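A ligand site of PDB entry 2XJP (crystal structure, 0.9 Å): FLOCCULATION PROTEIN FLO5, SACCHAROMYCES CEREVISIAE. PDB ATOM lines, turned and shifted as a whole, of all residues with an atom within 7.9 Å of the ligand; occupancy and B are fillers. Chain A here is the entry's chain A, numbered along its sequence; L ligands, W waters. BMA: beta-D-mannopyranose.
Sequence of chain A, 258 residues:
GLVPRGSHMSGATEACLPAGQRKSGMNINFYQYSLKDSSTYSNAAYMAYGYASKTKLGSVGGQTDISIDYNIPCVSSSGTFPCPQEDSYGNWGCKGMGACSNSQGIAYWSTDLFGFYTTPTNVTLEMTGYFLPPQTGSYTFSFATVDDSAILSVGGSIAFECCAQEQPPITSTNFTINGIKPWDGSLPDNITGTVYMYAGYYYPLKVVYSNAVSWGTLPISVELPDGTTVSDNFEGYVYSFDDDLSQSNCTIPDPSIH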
ATOM      1  N   ILE A  28      20.265  28.110   2.140  1.00  0.00           N
ATOM      2  CA  ILE A  28      21.443  27.267   2.331  1.00  0.00           C
ATOM      3  C   ILE A  28      22.134  27.711   3.594  1.00  0.00           C
ATOM      4  O   ILE A  28      22.598  28.838   3.707  1.00  0.00           O
ATOM      5  CB  ILE A  28      22.448  27.348   1.165  1.00  0.00           C
ATOM      6  CG1 ILE A  28      21.832  27.418  -0.203  1.00  0.00           C
ATOM      7  CG2 ILE A  28      23.497  26.255   1.335  1.00  0.00           C
ATOM      8  CD1 ILE A  28      21.133  26.224  -0.533  1.00  0.00           C
ATOM      9  N   PHE A  30      25.353  26.772   6.204  1.00  0.00           N
ATOM     10  CA  PHE A  30      26.662  26.165   6.162  1.00  0.00           C
ATOM     11  C   PHE A  30      27.151  25.900   7.572  1.00  0.00           C
ATOM     12  O   PHE A  30      27.003  26.752   8.451  1.00  0.00           O
ATOM     13  CB  PHE A  30      27.680  27.122   5.492  1.00  0.00           C
ATOM     14  CG  PHE A  30      27.376  27.418   4.071  1.00  0.00           C
ATOM     15  CD1 PHE A  30      28.012  26.730   3.050  1.00  0.00           C
ATOM     16  CD2 PHE A  30      26.443  28.385   3.693  1.00  0.00           C
ATOM     17  CE1 PHE A  30      27.775  27.017   1.732  1.00  0.00           C
ATOM     18  CE2 PHE A  30      26.173  28.678   2.377  1.00  0.00           C
ATOM     19  CZ  PHE A  30      26.867  27.999   1.388  1.00  0.00           C
ATOM     20  N   VAL A  60      22.989  31.605   2.980  1.00  0.00           N
ATOM     21  CA  VAL A  60      22.520  32.420   1.884  1.00  0.00           C
ATOM     22  C   VAL A  60      21.117  31.936   1.507  1.00  0.00           C
ATOM     23  O   VAL A  60      20.800  30.791   1.595  1.00  0.00           O
ATOM     24  CB  VAL A  60      23.423  32.315   0.629  1.00  0.00           C
ATOM     25  CG1 VAL A  60      24.882  32.653   0.845  1.00  0.00           C
ATOM     26  CG2 VAL A  60      23.435  30.935   0.089  1.00  0.00           C
ATOM     27  N   GLN A  63      18.265  30.560  -3.355  1.00  0.00           N
ATOM     28  CA  GLN A  63      19.070  29.831  -4.324  1.00  0.00           C
ATOM     29  C   GLN A  63      18.225  28.854  -5.130  1.00  0.00           C
ATOM     30  O   GLN A  63      17.592  27.962  -4.565  1.00  0.00           O
ATOM     31  CB  GLN A  63      20.194  29.064  -3.607  1.00  0.00           C
ATOM     32  CG  GLN A  63      21.110  30.015  -2.828  1.00  0.00           C
ATOM     33  CD  GLN A  63      21.770  31.042  -3.696  1.00  0.00           C
ATOM     34  OE1 GLN A  63      22.498  30.661  -4.619  1.00  0.00           O
ATOM     35  NE2 GLN A  63      21.555  32.308  -3.431  1.00  0.00           N
ATOM     36  N   THR A  64      18.244  29.014  -6.453  1.00  0.00           N
ATOM     37  CA  THR A  64      17.497  28.134  -7.332  1.00  0.00           C
ATOM     38  C   THR A  64      18.373  27.139  -8.086  1.00  0.00           C
ATOM     39  O   THR A  64      17.894  26.099  -8.494  1.00  0.00           O
ATOM     40  CB  THR A  64      16.655  28.931  -8.313  1.00  0.00           C
ATOM     41  OG1 THR A  64      17.491  29.847  -9.012  1.00  0.00           O
ATOM     42  CG2 THR A  64      15.557  29.678  -7.626  1.00  0.00           C
ATOM     43  N   ASP A  65      19.657  27.466  -8.238  1.00  0.00           N
ATOM     44  CA  ASP A  65      20.627  26.585  -8.885  1.00  0.00           C
ATOM     45  C   ASP A  65      21.366  25.878  -7.756  1.00  0.00           C
ATOM     46  O   ASP A  65      22.083  26.545  -6.993  1.00  0.00           O
ATOM     47  CB  ASP A  65      21.578  27.399  -9.745  1.00  0.00           C
ATOM     48  CG  ASP A  65      20.895  28.117 -10.892  1.00  0.00           C
ATOM     49  OD1 ASP A  65      20.484  27.443 -11.842  1.00  0.00           O
ATOM     50  OD2 ASP A  65      20.796  29.353 -10.893  1.00  0.00           O
ATOM     51  N   ILE A  66      21.102  24.583  -7.588  1.00  0.00           N
ATOM     52  CA  ILE A  66      21.429  23.881  -6.367  1.00  0.00           C
ATOM     53  C   ILE A  66      22.422  22.747  -6.495  1.00  0.00           C
ATOM     54  O   ILE A  66      22.814  22.160  -5.497  1.00  0.00           O
ATOM     55  CB  ILE A  66      20.156  23.392  -5.624  1.00  0.00           C
ATOM     56  CG1 ILE A  66      19.324  22.420  -6.454  1.00  0.00           C
ATOM     57  CG2 ILE A  66      19.386  24.644  -5.110  1.00  0.00           C
ATOM     58  CD1 ILE A  66      18.198  21.697  -5.701  1.00  0.00           C
ATOM     59  N   SER A  67      22.877  22.410  -7.701  1.00  0.00           N
ATOM     60  CA  SER A  67      23.894  21.372  -7.810  1.00  0.00           C
ATOM     61  C   SER A  67      25.249  21.883  -7.354  1.00  0.00           C
ATOM     62  O   SER A  67      25.571  23.072  -7.420  1.00  0.00           O
ATOM     63  CB  SER A  67      24.002  20.887  -9.245  1.00  0.00           C
ATOM     64  OG  SER A  67      22.835  20.121  -9.538  1.00  0.00           O
ATOM     65  N   ILE A  68      26.074  20.939  -6.920  1.00  0.00           N
ATOM     66  CA  ILE A  68      27.436  21.279  -6.477  1.00  0.00           C
ATOM     67  C   ILE A  68      28.424  20.629  -7.416  1.00  0.00           C
ATOM     68  O   ILE A  68      28.333  19.456  -7.772  1.00  0.00           O
ATOM     69  CB  ILE A  68      27.636  20.823  -5.041  1.00  0.00           C
ATOM     70  CG1 ILE A  68      26.660  21.631  -4.197  1.00  0.00           C
ATOM     71  CG2 ILE A  68      29.123  21.025  -4.569  1.00  0.00           C
ATOM     72  CD1 ILE A  68      26.528  21.032  -2.835  1.00  0.00           C
ATOM     73  N   ASP A  69      29.384  21.433  -7.803  1.00  0.00           N
ATOM     74  CA  ASP A  69      30.502  20.975  -8.661  1.00  0.00           C
ATOM     75  C   ASP A  69      31.712  21.806  -8.314  1.00  0.00           C
ATOM     76  O   ASP A  69      32.041  22.792  -8.970  1.00  0.00           O
ATOM     77  CB  ASP A  69      30.176  21.097 -10.161  1.00  0.00           C
ATOM     78  CG  ASP A  69      31.278  20.583 -11.024  1.00  0.00           C
ATOM     79  OD1 ASP A  69      32.177  19.910 -10.560  1.00  0.00           O
ATOM     80  OD2 ASP A  69      31.235  20.900 -12.219  1.00  0.00           O
ATOM     81  N   TYR A  70      32.378  21.451  -7.225  1.00  0.00           N
ATOM     82  CA  TYR A  70      33.514  22.170  -6.684  1.00  0.00           C
ATOM     83  C   TYR A  70      34.804  21.427  -7.101  1.00  0.00           C
ATOM     84  O   TYR A  70      34.974  20.251  -6.822  1.00  0.00           O
ATOM     85  CB  TYR A  70      33.447  22.250  -5.148  1.00  0.00           C
ATOM     86  CG  TYR A  70      34.726  22.801  -4.590  1.00  0.00           C
ATOM     87  CD1 TYR A  70      35.117  24.100  -4.838  1.00  0.00           C
ATOM     88  CD2 TYR A  70      35.622  21.974  -3.889  1.00  0.00           C
ATOM     89  CE1 TYR A  70      36.349  24.594  -4.400  1.00  0.00           C
ATOM     90  CE2 TYR A  70      36.836  22.437  -3.460  1.00  0.00           C
ATOM     91  CZ  TYR A  70      37.201  23.744  -3.719  1.00  0.00           C
ATOM     92  OH  TYR A  70      38.451  24.171  -3.295  1.00  0.00           O
ATOM     93  N   THR A 111      34.206  31.070  -3.069  1.00  0.00           N
ATOM     94  CA  THR A 111      32.775  31.351  -3.096  1.00  0.00           C
ATOM     95  C   THR A 111      31.980  30.397  -4.000  1.00  0.00           C
ATOM     96  O   THR A 111      30.807  30.654  -4.274  1.00  0.00           O
ATOM     97  CB  THR A 111      32.550  32.792  -3.574  1.00  0.00           C
ATOM     98  OG1 THR A 111      33.161  32.920  -4.872  1.00  0.00           O
ATOM     99  CG2 THR A 111      33.048  33.823  -2.582  1.00  0.00           C
ATOM    100  N   ASP A 112      32.593  29.310  -4.448  1.00  0.00           N
ATOM    101  CA  ASP A 112      31.945  28.371  -5.364  1.00  0.00           C
ATOM    102  C   ASP A 112      30.569  27.883  -4.883  1.00  0.00           C
ATOM    103  O   ASP A 112      29.703  27.625  -5.703  1.00  0.00           O
ATOM    104  CB  ASP A 112      32.857  27.171  -5.589  1.00  0.00           C
ATOM    105  CG  ASP A 112      32.391  26.322  -6.756  1.00  0.00           C
ATOM    106  OD1 ASP A 112      31.967  25.182  -6.469  1.00  0.00           O
ATOM    107  OD2 ASP A 112      32.349  26.867  -7.886  1.00  0.00           O
ATOM    108  N   LEU A 113      30.423  27.679  -3.587  1.00  0.00           N
ATOM    109  CA  LEU A 113      29.154  27.193  -3.035  1.00  0.00           C
ATOM    110  C   LEU A 113      28.260  28.387  -2.777  1.00  0.00           C
ATOM    111  O   LEU A 113      28.295  29.018  -1.721  1.00  0.00           O
ATOM    112  CB  LEU A 113      29.380  26.382  -1.795  1.00  0.00           C
ATOM    113  CG  LEU A 113      30.356  25.196  -1.919  1.00  0.00           C
ATOM    114  CD1 LEU A 113      30.551  24.542  -0.567  1.00  0.00           C
ATOM    115  CD2 LEU A 113      29.921  24.198  -2.952  1.00  0.00           C
ATOM    116  N   PHE A 114      27.411  28.727  -3.743  1.00  0.00           N
ATOM    117  CA  PHE A 114      26.299  29.686  -3.524  1.00  0.00           C
ATOM    118  C   PHE A 114      26.759  31.130  -3.295  1.00  0.00           C
ATOM    119  O   PHE A 114      25.968  31.941  -2.851  1.00  0.00           O
ATOM    120  CB  PHE A 114      25.314  29.193  -2.448  1.00  0.00           C
ATOM    121  CG  PHE A 114      24.785  27.822  -2.726  1.00  0.00           C
ATOM    122  CD1 PHE A 114      23.797  27.657  -3.643  1.00  0.00           C
ATOM    123  CD2 PHE A 114      25.308  26.706  -2.090  1.00  0.00           C
ATOM    124  CE1 PHE A 114      23.249  26.409  -3.916  1.00  0.00           C
ATOM    125  CE2 PHE A 114      24.843  25.462  -2.394  1.00  0.00           C
ATOM    126  CZ  PHE A 114      23.785  25.299  -3.305  1.00  0.00           C
ATOM    127  N   GLY A 115      28.003  31.455  -3.647  1.00  0.00           N
ATOM    128  CA  GLY A 115      28.535  32.779  -3.411  1.00  0.00           C
ATOM    129  C   GLY A 115      29.032  33.008  -1.990  1.00  0.00           C
ATOM    130  O   GLY A 115      29.520  34.100  -1.696  1.00  0.00           O
ATOM    131  N   PHE A 116      28.925  32.009  -1.119  1.00  0.00           N
ATOM    132  CA  PHE A 116      29.290  32.167   0.290  1.00  0.00           C
ATOM    133  C   PHE A 116      30.760  31.772   0.455  1.00  0.00           C
ATOM    134  O   PHE A 116      31.157  30.675   0.106  1.00  0.00           O
ATOM    135  CB  PHE A 116      28.419  31.230   1.162  1.00  0.00           C
ATOM    136  CG  PHE A 116      28.710  31.345   2.604  1.00  0.00           C
ATOM    137  CD1 PHE A 116      28.320  32.455   3.317  1.00  0.00           C
ATOM    138  CD2 PHE A 116      29.344  30.316   3.260  1.00  0.00           C
ATOM    139  CE1 PHE A 116      28.622  32.578   4.662  1.00  0.00           C
ATOM    140  CE2 PHE A 116      29.639  30.380   4.603  1.00  0.00           C
ATOM    141  CZ  PHE A 116      29.304  31.543   5.309  1.00  0.00           C
ATOM    142  N   LEU A 125      26.423  21.399   4.370  1.00  0.00           N
ATOM    143  CA  LEU A 125      25.486  22.459   4.126  1.00  0.00           C
ATOM    144  C   LEU A 125      24.134  21.799   4.000  1.00  0.00           C
ATOM    145  O   LEU A 125      23.991  20.657   3.577  1.00  0.00           O
ATOM    146  CB  LEU A 125      25.842  23.280   2.884  1.00  0.00           C
ATOM    147  CG  LEU A 125      25.962  22.504   1.546  1.00  0.00           C
ATOM    148  CD1 LEU A 125      24.584  22.328   0.867  1.00  0.00           C
ATOM    149  CD2 LEU A 125      26.934  23.204   0.604  1.00  0.00           C
ATOM    150  N   MET A 127      20.299  22.543   2.571  1.00  0.00           N
ATOM    151  CA  MET A 127      19.417  23.271   1.683  1.00  0.00           C
ATOM    152  C   MET A 127      17.995  22.976   2.154  1.00  0.00           C
ATOM    153  O   MET A 127      17.624  21.814   2.300  1.00  0.00           O
ATOM    154  CB  MET A 127      19.560  22.795   0.227  1.00  0.00           C
ATOM    155  CG  MET A 127      20.988  22.563  -0.207  1.00  0.00           C
ATOM    156  SD  MET A 127      20.997  22.220  -1.990  1.00  0.00           S
ATOM    157  CE  MET A 127      22.677  21.651  -2.208  1.00  0.00           C
ATOM    158  N   GLY A 216      34.248  18.291  -4.576  1.00  0.00           N
ATOM    159  CA  GLY A 216      32.892  18.114  -4.066  1.00  0.00           C
ATOM    160  C   GLY A 216      31.919  18.057  -5.225  1.00  0.00           C
ATOM    161  O   GLY A 216      31.996  18.901  -6.116  1.00  0.00           O
ATOM    162  N   LEU A 218      27.697  17.074  -6.370  1.00  0.00           N
ATOM    163  CA  LEU A 218      26.324  16.631  -6.072  1.00  0.00           C
ATOM    164  C   LEU A 218      25.417  17.189  -7.185  1.00  0.00           C
ATOM    165  O   LEU A 218      24.883  18.297  -7.089  1.00  0.00           O
ATOM    166  CB  LEU A 218      25.837  17.128  -4.721  1.00  0.00           C
ATOM    167  CG  LEU A 218      24.544  16.432  -4.274  1.00  0.00           C
ATOM    168  CD1 LEU A 218      24.759  14.955  -3.931  1.00  0.00           C
ATOM    169  CD2 LEU A 218      23.959  17.170  -3.069  1.00  0.00           C
ATOM    170  N   ASP A 232      19.724  20.699 -12.011  1.00  0.00           N
ATOM    171  CA  ASP A 232      20.599  21.763 -11.501  1.00  0.00           C
ATOM    172  C   ASP A 232      19.864  23.056 -11.195  1.00  0.00           C
ATOM    173  O   ASP A 232      19.893  23.532 -10.058  1.00  0.00           O
ATOM    174  CB  ASP A 232      21.814  21.974 -12.423  1.00  0.00           C
ATOM    175  CG  ASP A 232      22.461  20.648 -12.920  1.00  0.00           C
ATOM    176  OD1 ASP A 232      22.935  19.773 -12.121  1.00  0.00           O
ATOM    177  OD2 ASP A 232      22.562  20.489 -14.174  1.00  0.00           O
ATOM    178  N   ASN A 233      19.119  23.575 -12.187  1.00  0.00           N
ATOM    179  CA  ASN A 233      18.343  24.810 -12.094  1.00  0.00           C
ATOM    180  C   ASN A 233      16.905  24.435 -11.805  1.00  0.00           C
ATOM    181  O   ASN A 233      16.165  23.899 -12.653  1.00  0.00           O
ATOM    182  CB  ASN A 233      18.457  25.629 -13.379  1.00  0.00           C
ATOM    183  CG  ASN A 233      17.573  26.844 -13.395  1.00  0.00           C
ATOM    184  OD1 ASN A 233      16.990  27.230 -12.380  1.00  0.00           O
ATOM    185  ND2 ASN A 233      17.599  27.546 -14.510  1.00  0.00           N
HETATM  186  C1  BMA L   1      25.953  29.132  -6.993  1.00  0.00           C
HETATM  187  C2  BMA L   1      25.941  29.001  -8.516  1.00  0.00           C
HETATM  188  C3  BMA L   1      25.151  27.747  -8.866  1.00  0.00           C
HETATM  189  C4  BMA L   1      25.691  26.539  -8.098  1.00  0.00           C
HETATM  190  C5  BMA L   1      25.725  26.860  -6.614  1.00  0.00           C
HETATM  191  C6  BMA L   1      26.319  25.804  -5.701  1.00  0.00           C
HETATM  192  O1  BMA L   1      26.705  30.289  -6.629  1.00  0.00           O
HETATM  193  O2  BMA L   1      27.271  28.936  -8.992  1.00  0.00           O
HETATM  194  O3  BMA L   1      25.271  27.539 -10.252  1.00  0.00           O
HETATM  195  O4  BMA L   1      24.782  25.471  -8.374  1.00  0.00           O
HETATM  196  O5  BMA L   1      26.571  27.968  -6.401  1.00  0.00           O
HETATM  197  O6  BMA L   1      27.605  25.435  -6.013  1.00  0.00           O
HETATM  198  O   HOH W   1      29.500  27.745  -8.391  1.00  0.00           O
HETATM  199  O   HOH W   2      23.391  24.245 -10.314  1.00  0.00           O
HETATM  200  O   HOH W   3      29.324  30.839  -6.786  1.00  0.00           O
HETATM  201  O   HOH W   4      27.346  26.494 -11.269  1.00  0.00           O
HETATM  202  O   HOH W   5      29.613  24.063  -6.989  1.00  0.00           O
HETATM  203  O   HOH W   6      24.601  31.641  -6.079  1.00  0.00           O
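The backbone carbonyl oxygen of Ser 67 lies within hydrogen-bond range of an oxygen (O4) of the ligand (2.7 Å). An oxygen (O4) of the ligand sits at hydrogen-bond distance from the backbone carbonyl oxygen (O) of Asp 65, 3.2 Å away. The backbone carbonyl oxygen (O) of Asp 112 is in hydrogen-bond range of an oxygen (O6) of the ligand (3.0 Å). An oxygen (O1) of the ligand lies within hydrogen-bond range of the backbone NH of Gly 115, at 3.5 Å. The backbone NH of Phe 114 sits at hydrogen-bond distance from an oxygen (O5) of the ligand.
The backbone NH of Ile 66 sits at hydrogen-bond distance from the backbone carbonyl oxygen of Asp 232 (2.9 Å). The side-chain hydroxyl of Ser 67 sits at hydrogen-bond distance from the side-chain carboxylate of Asp 232.
Ile 66 touches the ligand (N to O4, 3.9 Å). Leu 113 touches the ligand (CA to O6, 3.8 Å). Hydrophobic or aromatic side chains within 4 Å of the ligand: Phe 114. Within 4 Å of the ligand: Asp 65, Ile 66, Ser 67, Asp 112, Leu 113, Phe 114 and Gly 115. Along chain A the residues within 4 Å of the ligand span positions 65 to 115. The nearest printed residue that does not touch the ligand is Ile 68 (4.2 Å).
Water W6 lies within hydrogen-bond range of an oxygen (O1) of the ligand (2.6 Å) and the side-chain amide oxygen of Gln 63 (2.7 Å). Water W1 bridges O2 of the ligand (2.6 Å) and O of Asp 112 (2.7 Å). Water W5 lies within hydrogen-bond range of an oxygen (O6) of the ligand (2.6 Å), the side-chain carboxylate (OD1) of Asp 112 (2.7 Å) and the backbone NH (N) of Asp 69 (2.8 Å). Water W3 lies within hydrogen-bond range of O1 of the ligand (2.7 Å), O of Thr 111 (2.9 Å), O of Asp 112 (3.4 Å) and N of Gly 115 (3.5 Å). Water W2 lies within hydrogen-bond range of an oxygen (O4) of the ligand (2.7 Å) and the backbone NH of Ser 67 (3.2 Å).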
